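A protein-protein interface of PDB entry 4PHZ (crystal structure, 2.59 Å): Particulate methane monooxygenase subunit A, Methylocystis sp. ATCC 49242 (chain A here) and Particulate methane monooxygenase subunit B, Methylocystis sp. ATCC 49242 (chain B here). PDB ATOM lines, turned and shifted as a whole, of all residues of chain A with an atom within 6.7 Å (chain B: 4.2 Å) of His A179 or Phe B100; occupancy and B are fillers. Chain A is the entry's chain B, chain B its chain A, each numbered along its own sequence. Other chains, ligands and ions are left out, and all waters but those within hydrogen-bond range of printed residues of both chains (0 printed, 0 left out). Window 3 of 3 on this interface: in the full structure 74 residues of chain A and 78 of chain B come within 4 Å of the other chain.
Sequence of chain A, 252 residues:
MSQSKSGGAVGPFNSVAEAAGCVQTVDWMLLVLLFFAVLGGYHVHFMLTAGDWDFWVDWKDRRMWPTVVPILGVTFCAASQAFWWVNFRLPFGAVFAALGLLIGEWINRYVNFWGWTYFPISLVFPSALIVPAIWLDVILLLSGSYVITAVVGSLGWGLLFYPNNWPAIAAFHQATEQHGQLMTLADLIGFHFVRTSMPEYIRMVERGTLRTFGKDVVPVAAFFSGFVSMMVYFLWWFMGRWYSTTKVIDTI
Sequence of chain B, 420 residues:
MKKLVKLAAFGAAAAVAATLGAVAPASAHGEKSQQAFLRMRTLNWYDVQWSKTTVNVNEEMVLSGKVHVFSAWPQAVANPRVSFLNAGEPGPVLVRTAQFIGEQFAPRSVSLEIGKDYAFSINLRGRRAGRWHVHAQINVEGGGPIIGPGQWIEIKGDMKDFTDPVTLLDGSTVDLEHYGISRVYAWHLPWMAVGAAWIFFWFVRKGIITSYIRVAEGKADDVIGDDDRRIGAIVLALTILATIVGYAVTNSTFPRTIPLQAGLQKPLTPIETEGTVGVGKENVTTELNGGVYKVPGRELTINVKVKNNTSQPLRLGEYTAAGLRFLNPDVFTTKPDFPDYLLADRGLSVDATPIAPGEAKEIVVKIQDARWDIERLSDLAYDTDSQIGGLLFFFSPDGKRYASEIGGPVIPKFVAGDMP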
ATOM      1  N   GLU A 177       5.013 -26.900   1.165  1.00  0.00           N
ATOM      2  CA  GLU A 177       4.975 -25.578   1.792  1.00  0.00           C
ATOM      3  C   GLU A 177       4.753 -24.463   0.757  1.00  0.00           C
ATOM      4  O   GLU A 177       5.602 -24.202  -0.100  1.00  0.00           O
ATOM      5  CB  GLU A 177       6.252 -25.295   2.588  1.00  0.00           C
ATOM      6  CG  GLU A 177       6.614 -23.808   2.571  1.00  0.00           C
ATOM      7  CD  GLU A 177       7.629 -23.385   3.617  1.00  0.00           C
ATOM      8  OE1 GLU A 177       8.330 -24.260   4.185  1.00  0.00           O
ATOM      9  OE2 GLU A 177       7.721 -22.157   3.864  1.00  0.00           O
ATOM     10  N   GLN A 178       3.604 -23.809   0.843  1.00  0.00           N
ATOM     11  CA  GLN A 178       3.363 -22.615   0.049  1.00  0.00           C
ATOM     12  C   GLN A 178       3.332 -21.462   1.008  1.00  0.00           C
ATOM     13  O   GLN A 178       2.750 -21.569   2.084  1.00  0.00           O
ATOM     14  CB  GLN A 178       2.037 -22.692  -0.697  1.00  0.00           C
ATOM     15  CG  GLN A 178       1.858 -23.980  -1.471  1.00  0.00           C
ATOM     16  CD  GLN A 178       2.768 -24.058  -2.675  1.00  0.00           C
ATOM     17  OE1 GLN A 178       3.637 -24.914  -2.731  1.00  0.00           O
ATOM     18  NE2 GLN A 178       2.565 -23.169  -3.651  1.00  0.00           N
ATOM     19  N   HIS A 179       3.984 -20.375   0.613  1.00  0.00           N
ATOM     20  CA  HIS A 179       4.025 -19.134   1.378  1.00  0.00           C
ATOM     21  C   HIS A 179       3.879 -19.325   2.861  1.00  0.00           C
ATOM     22  O   HIS A 179       2.965 -18.789   3.478  1.00  0.00           O
ATOM     23  CB  HIS A 179       2.978 -18.180   0.838  1.00  0.00           C
ATOM     24  CG  HIS A 179       3.092 -17.954  -0.640  1.00  0.00           C
ATOM     25  ND1 HIS A 179       3.690 -16.865  -1.156  1.00  0.00           N
ATOM     26  CD2 HIS A 179       2.684 -18.733  -1.720  1.00  0.00           C
ATOM     27  CE1 HIS A 179       3.664 -16.932  -2.505  1.00  0.00           C
ATOM     28  NE2 HIS A 179       3.046 -18.073  -2.850  1.00  0.00           N
ATOM     29  N   GLY A 180       4.774 -20.122   3.440  1.00  0.00           N
ATOM     30  CA  GLY A 180       4.835 -20.318   4.902  1.00  0.00           C
ATOM     31  C   GLY A 180       3.816 -21.268   5.519  1.00  0.00           C
ATOM     32  O   GLY A 180       3.884 -21.575   6.717  1.00  0.00           O
ATOM     33  N   GLN A 181       2.874 -21.734   4.698  1.00  0.00           N
ATOM     34  CA  GLN A 181       1.795 -22.628   5.123  1.00  0.00           C
ATOM     35  C   GLN A 181       2.028 -24.033   4.612  1.00  0.00           C
ATOM     36  O   GLN A 181       2.575 -24.247   3.524  1.00  0.00           O
ATOM     37  CB  GLN A 181       0.433 -22.135   4.603  1.00  0.00           C
ATOM     38  CG  GLN A 181      -0.381 -21.368   5.634  1.00  0.00           C
ATOM     39  CD  GLN A 181      -1.578 -20.654   5.024  1.00  0.00           C
ATOM     40  OE1 GLN A 181      -1.673 -19.418   5.074  1.00  0.00           O
ATOM     41  NE2 GLN A 181      -2.495 -21.421   4.438  1.00  0.00           N
ATOM     42  N   LEU A 182       1.594 -24.994   5.407  1.00  0.00           N
ATOM     43  CA  LEU A 182       1.526 -26.377   4.968  1.00  0.00           C
ATOM     44  C   LEU A 182       0.239 -26.645   4.165  1.00  0.00           C
ATOM     45  O   LEU A 182      -0.860 -26.245   4.571  1.00  0.00           O
ATOM     46  CB  LEU A 182       1.588 -27.292   6.181  1.00  0.00           C
ATOM     47  CG  LEU A 182       1.669 -28.774   5.869  1.00  0.00           C
ATOM     48  CD1 LEU A 182       2.886 -29.081   4.998  1.00  0.00           C
ATOM     49  CD2 LEU A 182       1.668 -29.569   7.172  1.00  0.00           C
ATOM     50  N   LEU B  85     -11.595 -15.216  -1.277  1.00  0.00           N
ATOM     51  CA  LEU B  85     -11.026 -14.476  -2.415  1.00  0.00           C
ATOM     52  C   LEU B  85     -10.888 -15.392  -3.604  1.00  0.00           C
ATOM     53  O   LEU B  85     -10.407 -16.498  -3.455  1.00  0.00           O
ATOM     54  CB  LEU B  85      -9.638 -13.931  -2.076  1.00  0.00           C
ATOM     55  CG  LEU B  85      -8.946 -13.166  -3.218  1.00  0.00           C
ATOM     56  CD1 LEU B  85      -9.736 -11.923  -3.643  1.00  0.00           C
ATOM     57  CD2 LEU B  85      -7.476 -12.872  -2.899  1.00  0.00           C
ATOM     58  N   ALA B  98      -0.981 -18.105  -6.212  1.00  0.00           N
ATOM     59  CA  ALA B  98      -1.149 -17.681  -4.830  1.00  0.00           C
ATOM     60  C   ALA B  98      -2.111 -16.523  -4.844  1.00  0.00           C
ATOM     61  O   ALA B  98      -2.407 -15.952  -5.905  1.00  0.00           O
ATOM     62  CB  ALA B  98       0.170 -17.277  -4.180  1.00  0.00           C
ATOM     63  N   GLN B  99      -2.626 -16.205  -3.663  1.00  0.00           N
ATOM     64  CA  GLN B  99      -3.461 -15.033  -3.493  1.00  0.00           C
ATOM     65  C   GLN B  99      -3.358 -14.557  -2.044  1.00  0.00           C
ATOM     66  O   GLN B  99      -2.996 -15.318  -1.135  1.00  0.00           O
ATOM     67  CB  GLN B  99      -4.909 -15.301  -3.914  1.00  0.00           C
ATOM     68  CG  GLN B  99      -5.581 -16.399  -3.105  1.00  0.00           C
ATOM     69  CD  GLN B  99      -7.051 -16.567  -3.419  1.00  0.00           C
ATOM     70  OE1 GLN B  99      -7.539 -16.095  -4.446  1.00  0.00           O
ATOM     71  NE2 GLN B  99      -7.767 -17.236  -2.532  1.00  0.00           N
ATOM     72  N   PHE B 100      -3.652 -13.282  -1.854  1.00  0.00           N
ATOM     73  CA  PHE B 100      -3.407 -12.622  -0.596  1.00  0.00           C
ATOM     74  C   PHE B 100      -4.520 -11.640  -0.371  1.00  0.00           C
ATOM     75  O   PHE B 100      -5.076 -11.079  -1.321  1.00  0.00           O
ATOM     76  CB  PHE B 100      -2.074 -11.885  -0.645  1.00  0.00           C
ATOM     77  CG  PHE B 100      -0.907 -12.778  -0.944  1.00  0.00           C
ATOM     78  CD1 PHE B 100      -0.504 -13.013  -2.276  1.00  0.00           C
ATOM     79  CD2 PHE B 100      -0.209 -13.402   0.097  1.00  0.00           C
ATOM     80  CE1 PHE B 100       0.569 -13.864  -2.554  1.00  0.00           C
ATOM     81  CE2 PHE B 100       0.864 -14.240  -0.176  1.00  0.00           C
ATOM     82  CZ  PHE B 100       1.253 -14.476  -1.498  1.00  0.00           C
ATOM     83  N   ILE B 101      -4.858 -11.444   0.893  1.00  0.00           N
ATOM     84  CA  ILE B 101      -5.830 -10.413   1.268  1.00  0.00           C
ATOM     85  C   ILE B 101      -5.635 -10.159   2.747  1.00  0.00           C
ATOM     86  O   ILE B 101      -5.315 -11.083   3.492  1.00  0.00           O
ATOM     87  CB  ILE B 101      -7.292 -10.828   0.952  1.00  0.00           C
ATOM     88  CG1 ILE B 101      -8.261  -9.716   1.348  1.00  0.00           C
ATOM     89  CG2 ILE B 101      -7.646 -12.135   1.654  1.00  0.00           C
ATOM     90  CD1 ILE B 101      -9.557  -9.703   0.567  1.00  0.00           C
ATOM     91  N   GLN B 104      -2.528 -11.320   4.217  1.00  0.00           N
ATOM     92  CA  GLN B 104      -2.395 -12.763   4.453  1.00  0.00           C
ATOM     93  C   GLN B 104      -2.499 -13.571   3.165  1.00  0.00           C
ATOM     94  O   GLN B 104      -3.241 -13.212   2.232  1.00  0.00           O
ATOM     95  CB  GLN B 104      -3.465 -13.261   5.397  1.00  0.00           C
ATOM     96  CG  GLN B 104      -3.111 -13.180   6.858  1.00  0.00           C
ATOM     97  CD  GLN B 104      -4.301 -13.559   7.705  1.00  0.00           C
ATOM     98  OE1 GLN B 104      -4.788 -12.758   8.502  1.00  0.00           O
ATOM     99  NE2 GLN B 104      -4.803 -14.777   7.511  1.00  0.00           N
ATOM    100  N   PHE B 105      -1.715 -14.647   3.138  1.00  0.00           N
ATOM    101  CA  PHE B 105      -1.779 -15.653   2.104  1.00  0.00           C
ATOM    102  C   PHE B 105      -3.105 -16.354   2.356  1.00  0.00           C
ATOM    103  O   PHE B 105      -3.338 -16.853   3.458  1.00  0.00           O
ATOM    104  CB  PHE B 105      -0.566 -16.616   2.205  1.00  0.00           C
ATOM    105  CG  PHE B 105      -0.650 -17.806   1.286  1.00  0.00           C
ATOM    106  CD1 PHE B 105      -0.901 -17.642  -0.086  1.00  0.00           C
ATOM    107  CD2 PHE B 105      -0.476 -19.103   1.793  1.00  0.00           C
ATOM    108  CE1 PHE B 105      -0.998 -18.758  -0.926  1.00  0.00           C
ATOM    109  CE2 PHE B 105      -0.575 -20.203   0.964  1.00  0.00           C
ATOM    110  CZ  PHE B 105      -0.843 -20.030  -0.394  1.00  0.00           C
ATOM    111  N   PHE B 120      -5.996  -6.881  -1.720  1.00  0.00           N
ATOM    112  CA  PHE B 120      -5.797  -8.261  -2.137  1.00  0.00           C
ATOM    113  C   PHE B 120      -5.023  -8.316  -3.442  1.00  0.00           C
ATOM    114  O   PHE B 120      -5.010  -7.352  -4.223  1.00  0.00           O
ATOM    115  CB  PHE B 120      -7.146  -8.913  -2.374  1.00  0.00           C
ATOM    116  CG  PHE B 120      -7.918  -8.268  -3.477  1.00  0.00           C
ATOM    117  CD1 PHE B 120      -7.691  -8.634  -4.800  1.00  0.00           C
ATOM    118  CD2 PHE B 120      -8.842  -7.265  -3.199  1.00  0.00           C
ATOM    119  CE1 PHE B 120      -8.387  -8.020  -5.830  1.00  0.00           C
ATOM    120  CE2 PHE B 120      -9.545  -6.651  -4.227  1.00  0.00           C
ATOM    121  CZ  PHE B 120      -9.321  -7.028  -5.543  1.00  0.00           C
ATOM    122  N   SER B 121      -4.405  -9.459  -3.693  1.00  0.00           N
ATOM    123  CA  SER B 121      -3.860  -9.725  -5.012  1.00  0.00           C
ATOM    124  C   SER B 121      -3.789 -11.219  -5.257  1.00  0.00           C
ATOM    125  O   SER B 121      -3.689 -12.020  -4.317  1.00  0.00           O
ATOM    126  CB  SER B 121      -2.492  -9.067  -5.215  1.00  0.00           C
ATOM    127  OG  SER B 121      -1.602  -9.495  -4.212  1.00  0.00           O
ATOM    128  N   ASN B 123      -2.054 -14.063  -7.939  1.00  0.00           N
ATOM    129  CA  ASN B 123      -1.084 -14.401  -8.960  1.00  0.00           C
ATOM    130  C   ASN B 123      -1.664 -15.423  -9.940  1.00  0.00           C
ATOM    131  O   ASN B 123      -1.856 -16.607  -9.588  1.00  0.00           O
ATOM    132  CB  ASN B 123       0.195 -14.969  -8.321  1.00  0.00           C
ATOM    133  CG  ASN B 123       0.873 -13.986  -7.404  1.00  0.00           C
ATOM    134  OD1 ASN B 123       0.861 -12.791  -7.656  1.00  0.00           O
ATOM    135  ND2 ASN B 123       1.465 -14.483  -6.325  1.00  0.00           N
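The backbone NH (N) of Phe B100 is in hydrogen-bond range of the backbone carbonyl oxygen (O) of Ser B121, 2.8 Å away. O of Ala B98 sits at hydrogen-bond distance from N of Asn B123 (2.8 Å).
Of chain B, only Ala B98 (3.3 Å), Phe B100 (3.4 Å) and Phe B105 (3.7 Å) come within 4 Å of His A179. Printed residues of chain B within 4 Å of Gln A178: Phe B105. Printed residues of chain A within 4 Å of Phe B105: Gln A178, His A179 and Gln A181. Of the printed residues of chain B, Gln A181 touches Phe B105 (3.5 Å). Of the printed residues of chain A, Ala B98 touches His A179 (3.3 Å). Gly A180 touches none of the printed residues of chain B. Gln B104 touches none of the printed residues of chain A. The nearest printed residue of chain B that does not touch His A179 is Asn B123 (5.0 Å).
Phe B105 touches Gln A178. Ala B98 touches His A179. CZ of Phe B100 touches ND1 of His A179, at 3.4 Å. His A179 touches Phe B105 (CB to CG, 3.7 Å).
Printed residues of chain A that touch a printed residue of chain B: Gln A178, His A179 and Gln A181. Hydrophobic or aromatic side chains of chain A within 4 Å of the printed part of chain B: His A179. Of the 10 printed residues of chain B, 3 touch a printed residue of chain A. Printed residues of chain B that touch a printed residue of chain A: Ala B98, Phe B100 and Phe B105. Among the printed residues, 5 pairs touch across the chains. Among the printed residues, no Asp or Glu carboxylate lies within 4 Å of a Lys or Arg side-chain nitrogen of the other chain.
The side-chain amide oxygen (OE1) of Gln A181 lies close to the backbone carbonyl oxygen (O) of Phe B105 (3.5 Å).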
